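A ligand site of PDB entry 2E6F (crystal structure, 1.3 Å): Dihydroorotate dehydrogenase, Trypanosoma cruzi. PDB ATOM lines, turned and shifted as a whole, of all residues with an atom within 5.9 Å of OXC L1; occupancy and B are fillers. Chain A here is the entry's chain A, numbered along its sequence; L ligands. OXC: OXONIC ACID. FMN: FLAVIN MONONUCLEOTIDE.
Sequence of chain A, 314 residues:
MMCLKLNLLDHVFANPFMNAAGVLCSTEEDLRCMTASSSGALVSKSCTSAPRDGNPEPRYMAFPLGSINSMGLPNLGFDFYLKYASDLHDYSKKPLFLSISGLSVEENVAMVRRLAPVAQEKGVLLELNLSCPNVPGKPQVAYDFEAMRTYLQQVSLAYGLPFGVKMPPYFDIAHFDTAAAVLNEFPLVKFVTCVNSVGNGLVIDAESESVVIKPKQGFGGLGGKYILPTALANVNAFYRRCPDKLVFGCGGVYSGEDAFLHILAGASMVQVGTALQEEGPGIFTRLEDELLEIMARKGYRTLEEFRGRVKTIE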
ATOM      1  N   LYS A  45     -16.838  -7.970  31.569  1.00  0.00           N
ATOM      2  CA  LYS A  45     -15.457  -7.933  31.092  1.00  0.00           C
ATOM      3  C   LYS A  45     -14.921  -9.334  30.857  1.00  0.00           C
ATOM      4  O   LYS A  45     -15.108 -10.218  31.700  1.00  0.00           O
ATOM      5  CB  LYS A  45     -14.588  -7.222  32.140  1.00  0.00           C
ATOM      6  CG  LYS A  45     -13.083  -7.330  31.923  1.00  0.00           C
ATOM      7  CD  LYS A  45     -12.660  -6.544  30.683  1.00  0.00           C
ATOM      8  CE  LYS A  45     -11.217  -6.817  30.263  1.00  0.00           C
ATOM      9  NZ  LYS A  45     -10.906  -6.088  29.002  1.00  0.00           N
ATOM     10  N   SER A  46     -14.237  -9.557  29.736  1.00  0.00           N
ATOM     11  CA  SER A  46     -13.611 -10.855  29.507  1.00  0.00           C
ATOM     12  C   SER A  46     -12.710 -11.206  30.672  1.00  0.00           C
ATOM     13  O   SER A  46     -11.827 -10.415  31.043  1.00  0.00           O
ATOM     14  CB  SER A  46     -12.792 -10.865  28.221  1.00  0.00           C
ATOM     15  OG  SER A  46     -13.614 -10.912  27.080  1.00  0.00           O
ATOM     16  N   ASN A  55      -2.094  -4.739  31.168  1.00  0.00           N
ATOM     17  CA  ASN A  55      -0.868  -4.127  30.631  1.00  0.00           C
ATOM     18  C   ASN A  55      -0.595  -2.752  31.272  1.00  0.00           C
ATOM     19  O   ASN A  55      -1.489  -2.164  31.865  1.00  0.00           O
ATOM     20  CB  ASN A  55      -1.006  -3.981  29.123  1.00  0.00           C
ATOM     21  CG  ASN A  55      -1.020  -5.308  28.378  1.00  0.00           C
ATOM     22  OD1 ASN A  55      -0.607  -6.345  28.911  1.00  0.00           O
ATOM     23  ND2 ASN A  55      -1.486  -5.275  27.150  1.00  0.00           N
ATOM     24  N   ASN A  69      -6.428   0.599  22.001  1.00  0.00           N
ATOM     25  CA  ASN A  69      -6.283   0.065  23.346  1.00  0.00           C
ATOM     26  C   ASN A  69      -5.362  -1.133  23.369  1.00  0.00           C
ATOM     27  O   ASN A  69      -5.316  -1.921  22.416  1.00  0.00           O
ATOM     28  CB  ASN A  69      -7.650  -0.272  23.972  1.00  0.00           C
ATOM     29  CG  ASN A  69      -8.052  -1.729  23.784  1.00  0.00           C
ATOM     30  OD1 ASN A  69      -7.530  -2.625  24.474  1.00  0.00           O
ATOM     31  ND2 ASN A  69      -8.976  -1.981  22.870  1.00  0.00           N
ATOM     32  N   SER A  70      -4.605  -1.261  24.446  1.00  0.00           N
ATOM     33  CA  SER A  70      -3.943  -2.520  24.776  1.00  0.00           C
ATOM     34  C   SER A  70      -4.170  -2.814  26.251  1.00  0.00           C
ATOM     35  O   SER A  70      -3.238  -2.795  27.057  1.00  0.00           O
ATOM     36  CB  SER A  70      -2.458  -2.479  24.431  1.00  0.00           C
ATOM     37  OG  SER A  70      -1.853  -3.750  24.654  1.00  0.00           O
ATOM     38  N   MET A  71      -5.422  -3.087  26.610  1.00  0.00           N
ATOM     39  CA  MET A  71      -5.767  -3.237  28.024  1.00  0.00           C
ATOM     40  C   MET A  71      -5.023  -4.395  28.669  1.00  0.00           C
ATOM     41  O   MET A  71      -4.485  -4.258  29.768  1.00  0.00           O
ATOM     42  CB  MET A  71      -7.276  -3.414  28.235  1.00  0.00           C
ATOM     43  CG  MET A  71      -8.156  -2.295  27.671  1.00  0.00           C
ATOM     44  SD  MET A  71      -7.759  -0.631  28.221  1.00  0.00           S
ATOM     45  CE  MET A  71      -8.331  -0.672  29.911  1.00  0.00           C
ATOM     46  N   GLY A  72      -4.987  -5.529  27.971  1.00  0.00           N
ATOM     47  CA  GLY A  72      -4.320  -6.734  28.455  1.00  0.00           C
ATOM     48  C   GLY A  72      -5.156  -7.572  29.408  1.00  0.00           C
ATOM     49  O   GLY A  72      -4.619  -8.204  30.323  1.00  0.00           O
ATOM     50  N   LEU A  73      -6.469  -7.584  29.182  1.00  0.00           N
ATOM     51  CA  LEU A  73      -7.428  -8.329  30.013  1.00  0.00           C
ATOM     52  C   LEU A  73      -7.348  -8.020  31.519  1.00  0.00           C
ATOM     53  O   LEU A  73      -7.352  -8.947  32.332  1.00  0.00           O
ATOM     54  CB  LEU A  73      -7.346  -9.834  29.753  1.00  0.00           C
ATOM     55  CG  LEU A  73      -7.713 -10.306  28.346  1.00  0.00           C
ATOM     56  CD1 LEU A  73      -7.382 -11.779  28.187  1.00  0.00           C
ATOM     57  CD2 LEU A  73      -9.192 -10.052  28.047  1.00  0.00           C
ATOM     58  N   PRO A  74      -7.321  -6.729  31.901  1.00  0.00           N
ATOM     59  CA  PRO A  74      -7.417  -6.429  33.320  1.00  0.00           C
ATOM     60  C   PRO A  74      -8.810  -6.848  33.769  1.00  0.00           C
ATOM     61  O   PRO A  74      -9.796  -6.496  33.132  1.00  0.00           O
ATOM     62  CB  PRO A  74      -7.245  -4.913  33.395  1.00  0.00           C
ATOM     63  CG  PRO A  74      -7.623  -4.402  32.037  1.00  0.00           C
ATOM     64  CD  PRO A  74      -7.303  -5.511  31.068  1.00  0.00           C
ATOM     65  N   SER A 101     -12.101 -15.192  28.558  1.00  0.00           N
ATOM     66  CA  SER A 101     -10.976 -15.115  27.638  1.00  0.00           C
ATOM     67  C   SER A 101      -9.737 -15.741  28.242  1.00  0.00           C
ATOM     68  O   SER A 101      -8.752 -15.069  28.508  1.00  0.00           O
ATOM     69  CB  SER A 101     -10.722 -13.659  27.241  1.00  0.00           C
ATOM     70  OG  SER A 101      -9.885 -13.588  26.115  1.00  0.00           O
ATOM     71  N   ASN A 129     -14.427 -15.563  24.164  1.00  0.00           N
ATOM     72  CA  ASN A 129     -13.591 -14.613  23.439  1.00  0.00           C
ATOM     73  C   ASN A 129     -12.400 -15.299  22.767  1.00  0.00           C
ATOM     74  O   ASN A 129     -11.460 -15.710  23.434  1.00  0.00           O
ATOM     75  CB  ASN A 129     -13.115 -13.508  24.404  1.00  0.00           C
ATOM     76  CG  ASN A 129     -12.308 -12.423  23.725  1.00  0.00           C
ATOM     77  OD1 ASN A 129     -11.997 -12.498  22.526  1.00  0.00           O
ATOM     78  ND2 ASN A 129     -11.956 -11.408  24.483  1.00  0.00           N
ATOM     79  N   SER A 131     -10.576 -13.763  20.380  1.00  0.00           N
ATOM     80  CA  SER A 131     -10.055 -12.698  19.549  1.00  0.00           C
ATOM     81  C   SER A 131      -9.327 -11.570  20.275  1.00  0.00           C
ATOM     82  O   SER A 131      -9.055 -10.537  19.681  1.00  0.00           O
ATOM     83  CB  SER A 131     -11.167 -12.138  18.649  1.00  0.00           C
ATOM     84  OG  SER A 131     -12.355 -11.908  19.384  1.00  0.00           O
ATOM     85  N   CYS A 132      -8.968 -11.776  21.539  1.00  0.00           N
ATOM     86  CA  CYS A 132      -8.170 -10.771  22.247  1.00  0.00           C
ATOM     87  C   CYS A 132      -6.845 -10.535  21.503  1.00  0.00           C
ATOM     88  O   CYS A 132      -6.082 -11.486  21.304  1.00  0.00           O
ATOM     89  CB  CYS A 132      -7.881 -11.201  23.685  1.00  0.00           C
ATOM     90  SG  CYS A 132      -6.906  -9.963  24.605  1.00  0.00           S
ATOM     91  N   PRO A 133      -6.575  -9.272  21.089  1.00  0.00           N
ATOM     92  CA  PRO A 133      -5.358  -8.977  20.348  1.00  0.00           C
ATOM     93  C   PRO A 133      -4.252  -8.290  21.166  1.00  0.00           C
ATOM     94  O   PRO A 133      -3.296  -7.772  20.569  1.00  0.00           O
ATOM     95  CB  PRO A 133      -5.873  -8.013  19.292  1.00  0.00           C
ATOM     96  CG  PRO A 133      -6.878  -7.168  20.070  1.00  0.00           C
ATOM     97  CD  PRO A 133      -7.446  -8.085  21.155  1.00  0.00           C
ATOM     98  N   ASN A 134      -4.369  -8.286  22.491  1.00  0.00           N
ATOM     99  CA  ASN A 134      -3.541  -7.408  23.343  1.00  0.00           C
ATOM    100  C   ASN A 134      -2.671  -8.067  24.408  1.00  0.00           C
ATOM    101  O   ASN A 134      -1.911  -7.356  25.070  1.00  0.00           O
ATOM    102  CB  ASN A 134      -4.422  -6.347  24.025  1.00  0.00           C
ATOM    103  CG  ASN A 134      -5.123  -5.438  23.047  1.00  0.00           C
ATOM    104  OD1 ASN A 134      -4.560  -5.053  22.022  1.00  0.00           O
ATOM    105  ND2 ASN A 134      -6.350  -5.047  23.375  1.00  0.00           N
ATOM    106  N   VAL A 135      -2.749  -9.379  24.597  1.00  0.00           N
ATOM    107  CA  VAL A 135      -1.886 -10.006  25.610  1.00  0.00           C
ATOM    108  C   VAL A 135      -0.553 -10.352  24.945  1.00  0.00           C
ATOM    109  O   VAL A 135      -0.537 -11.061  23.925  1.00  0.00           O
ATOM    110  CB  VAL A 135      -2.535 -11.249  26.262  1.00  0.00           C
ATOM    111  CG1 VAL A 135      -1.558 -11.911  27.247  1.00  0.00           C
ATOM    112  CG2 VAL A 135      -3.815 -10.868  26.980  1.00  0.00           C
ATOM    113  N   LYS A 166     -16.928 -14.555  20.387  1.00  0.00           N
ATOM    114  CA  LYS A 166     -16.448 -13.234  19.959  1.00  0.00           C
ATOM    115  C   LYS A 166     -15.314 -13.433  18.954  1.00  0.00           C
ATOM    116  O   LYS A 166     -14.245 -13.950  19.294  1.00  0.00           O
ATOM    117  CB  LYS A 166     -15.973 -12.419  21.162  1.00  0.00           C
ATOM    118  CG  LYS A 166     -15.535 -10.982  20.850  1.00  0.00           C
ATOM    119  CD  LYS A 166     -16.709 -10.085  20.465  1.00  0.00           C
ATOM    120  CE  LYS A 166     -16.325  -8.610  20.435  1.00  0.00           C
ATOM    121  NZ  LYS A 166     -16.088  -8.050  21.788  1.00  0.00           N
ATOM    122  N   ASN A 196     -14.448  -8.181  17.332  1.00  0.00           N
ATOM    123  CA  ASN A 196     -13.497  -7.616  18.284  1.00  0.00           C
ATOM    124  C   ASN A 196     -12.702  -6.483  17.618  1.00  0.00           C
ATOM    125  O   ASN A 196     -12.862  -6.215  16.408  1.00  0.00           O
ATOM    126  CB  ASN A 196     -12.583  -8.741  18.784  1.00  0.00           C
ATOM    127  CG  ASN A 196     -12.071  -8.507  20.205  1.00  0.00           C
ATOM    128  OD1 ASN A 196     -11.639  -7.409  20.560  1.00  0.00           O
ATOM    129  ND2 ASN A 196     -12.119  -9.555  21.029  1.00  0.00           N
ATOM    130  N   SER A 197     -11.860  -5.794  18.390  1.00  0.00           N
ATOM    131  CA  SER A 197     -11.086  -4.687  17.860  1.00  0.00           C
ATOM    132  C   SER A 197     -10.171  -5.138  16.722  1.00  0.00           C
ATOM    133  O   SER A 197      -9.770  -6.309  16.640  1.00  0.00           O
ATOM    134  CB  SER A 197     -10.281  -3.990  18.963  1.00  0.00           C
ATOM    135  OG  SER A 197      -9.369  -4.901  19.569  1.00  0.00           O
ATOM    136  N   GLY A 221      -5.440  -2.600  19.714  1.00  0.00           N
ATOM    137  CA  GLY A 221      -6.655  -2.840  18.933  1.00  0.00           C
ATOM    138  C   GLY A 221      -7.409  -1.550  18.656  1.00  0.00           C
ATOM    139  O   GLY A 221      -7.519  -0.694  19.532  1.00  0.00           O
HETATM  140  N1  OXC L   1     -10.312  -6.917  22.912  1.00  0.00           N
HETATM  141  C2  OXC L   1      -9.742  -5.715  23.160  1.00  0.00           C
HETATM  142  O2  OXC L   1      -9.859  -4.774  22.336  1.00  0.00           O
HETATM  143  N3  OXC L   1      -9.055  -5.533  24.309  1.00  0.00           N
HETATM  144  C4  OXC L   1      -8.956  -6.568  25.176  1.00  0.00           C
HETATM  145  N5  OXC L   1      -9.508  -7.786  24.934  1.00  0.00           N
HETATM  146  C6  OXC L   1     -10.198  -7.958  23.784  1.00  0.00           C
HETATM  147  O6  OXC L   1     -10.721  -9.059  23.515  1.00  0.00           O
HETATM  148  CG  OXC L   1      -8.122  -6.406  26.403  1.00  0.00           C
HETATM  149  OD1 OXC L   1      -8.593  -6.507  27.550  1.00  0.00           O
HETATM  150  OD2 OXC L   1      -6.910  -6.228  26.147  1.00  0.00           O
HETATM  151  N1  FMN L   2     -13.655  -7.291  23.620  1.00  0.00           N
HETATM  152  C2  FMN L   2     -13.791  -8.494  24.271  1.00  0.00           C
HETATM  153  O2  FMN L   2     -14.302  -9.455  23.682  1.00  0.00           O
HETATM  154  N3  FMN L   2     -13.385  -8.615  25.588  1.00  0.00           N
HETATM  155  C4  FMN L   2     -12.833  -7.563  26.285  1.00  0.00           C
HETATM  156  O4  FMN L   2     -12.680  -7.665  27.510  1.00  0.00           O
HETATM  157  C4A FMN L   2     -12.699  -6.351  25.635  1.00  0.00           C
HETATM  158  N5  FMN L   2     -12.172  -5.263  26.296  1.00  0.00           N
HETATM  159  C5A FMN L   2     -12.097  -4.048  25.645  1.00  0.00           C
HETATM  160  C6  FMN L   2     -11.581  -2.944  26.320  1.00  0.00           C
HETATM  161  C7  FMN L   2     -11.505  -1.699  25.700  1.00  0.00           C
HETATM  162  C7M FMN L   2     -11.343  -0.491  26.579  1.00  0.00           C
HETATM  163  C8  FMN L   2     -11.924  -1.571  24.355  1.00  0.00           C
HETATM  164  C8M FMN L   2     -12.200  -0.212  23.767  1.00  0.00           C
HETATM  165  C9  FMN L   2     -12.436  -2.685  23.679  1.00  0.00           C
HETATM  166  C9A FMN L   2     -12.527  -3.925  24.326  1.00  0.00           C
HETATM  167  N10 FMN L   2     -13.021  -5.022  23.653  1.00  0.00           N
HETATM  168  C10 FMN L   2     -13.133  -6.228  24.306  1.00  0.00           C
HETATM  169  C1' FMN L   2     -13.374  -4.939  22.202  1.00  0.00           C
HETATM  170  C2' FMN L   2     -14.805  -4.440  22.108  1.00  0.00           C
HETATM  171  O2' FMN L   2     -15.678  -5.364  22.728  1.00  0.00           O
HETATM  172  C3' FMN L   2     -15.244  -4.237  20.660  1.00  0.00           C
HETATM  173  O3' FMN L   2     -15.213  -5.504  20.034  1.00  0.00           O
HETATM  174  C4' FMN L   2     -14.367  -3.250  19.898  1.00  0.00           C
HETATM  175  O4' FMN L   2     -13.982  -2.178  20.737  1.00  0.00           O
HETATM  176  C5' FMN L   2     -15.041  -2.735  18.623  1.00  0.00           C
HETATM  177  O5' FMN L   2     -16.253  -2.053  18.930  1.00  0.00           O
HETATM  178  P   FMN L   2     -16.332  -0.446  18.930  1.00  0.00           P
HETATM  179  O1P FMN L   2     -15.995   0.047  17.544  1.00  0.00           O
HETATM  180  O2P FMN L   2     -17.745  -0.100  19.346  1.00  0.00           O
HETATM  181  O3P FMN L   2     -15.312   0.065  19.924  1.00  0.00           O
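The backbone NH (N) of Gly 72 lies within hydrogen-bond range of an oxygen (OD2) of OXC L1.
The side-chain amide oxygen (OD1) of Asn 196 lies within hydrogen-bond range of a nitrogen (N1) of OXC L1, 2.7 Å away.
An oxygen (OD1) of OXC L1 lies within salt-bridge range of the side-chain amino group of Lys 45 (2.8 Å).
The side-chain hydroxyl of Ser 197 lies within hydrogen-bond range of an oxygen (O2) of OXC L1 (2.8 Å).
O6 of OXC L1 sits at hydrogen-bond distance from ND2 of Asn 129.
An oxygen (OD1) of OXC L1 is in hydrogen-bond range of the backbone NH of Leu 73, 2.9 Å away.
The side-chain amide nitrogen of Asn 134 lies close to a nitrogen (N3) of OXC L1 (2.9 Å).
An oxygen (O2) of OXC L1 sits at hydrogen-bond distance from the side-chain amide nitrogen (ND2) of Asn 69, at 3.0 Å.
SG of Cys 132 sits at hydrogen-bond distance from N5 of OXC L1 (3.4 Å).
O2 of FMN L2 sits at hydrogen-bond distance from ND2 of Asn 196, 3.4 Å away.
The side-chain amino group (NZ) of Lys 45 lies within hydrogen-bond range of an oxygen (O4) of FMN L2, 2.8 Å away.
ND2 of Asn 129 lies within hydrogen-bond range of O2 of FMN L2, at 3.2 Å.
An oxygen (O4) of FMN L2 sits close to the backbone NH (N) of Ser 46.
The side-chain hydroxyl (OG) of Ser 46 is in hydrogen-bond range of a nitrogen (N3) of FMN L2, at 2.7 Å.
O2' of FMN L2 is in hydrogen-bond range of NZ of Lys 166 (2.9 Å).
An oxygen (O6) of OXC L1 sits close to a nitrogen (N3) of FMN L2, 3.4 Å away.
Met 71 touches OXC L1.
CD of Pro 74 touches OD1 of OXC L1 (3.9 Å).
CD of Pro 133 touches N1 of OXC L1, 3.6 Å away.
Hydrophobic or aromatic side chains that line OXC L1: Met 71, Leu 73, Pro 74 and Pro 133.
12 residues have an atom within 4 Å of OXC L1: Lys 45, Asn 69, Met 71, Gly 72, Leu 73, Pro 74, Asn 129, Cys 132, Pro 133, Asn 134, Asn 196 and Ser 197.
Along chain A the residues within 4 Å of OXC L1 span positions 45 to 197.
The nearest printed residue that does not touch OXC L1 is Ser 131 (4.3 Å).
The side-chain amide oxygen (OD1) of Asn 129 lies within hydrogen-bond range of the side-chain amide nitrogen (ND2) of Asn 196 (3.3 Å).
The side-chain amide nitrogen (ND2) of Asn 196 lies within hydrogen-bond range of the side-chain hydroxyl (OG) of Ser 131, 2.9 Å away.
The backbone NH (N) of Ser 131 lies within hydrogen-bond range of the side-chain amide oxygen (OD1) of Asn 129.
ND2 of Asn 134 lies within hydrogen-bond range of OD1 of Asn 69, 2.9 Å away.
N of Asn 134 lies close to SG of Cys 132, 3.7 Å away.
The backbone carbonyl oxygen (O) of Asn 134 lies within hydrogen-bond range of the side-chain amide nitrogen (ND2) of Asn 55.
N of Met 71 lies within hydrogen-bond range of OD1 of Asn 69, at 3.0 Å.
The backbone NH (N) of Asn 55 sits at hydrogen-bond distance from the backbone carbonyl oxygen (O) of Met 71 (2.8 Å).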
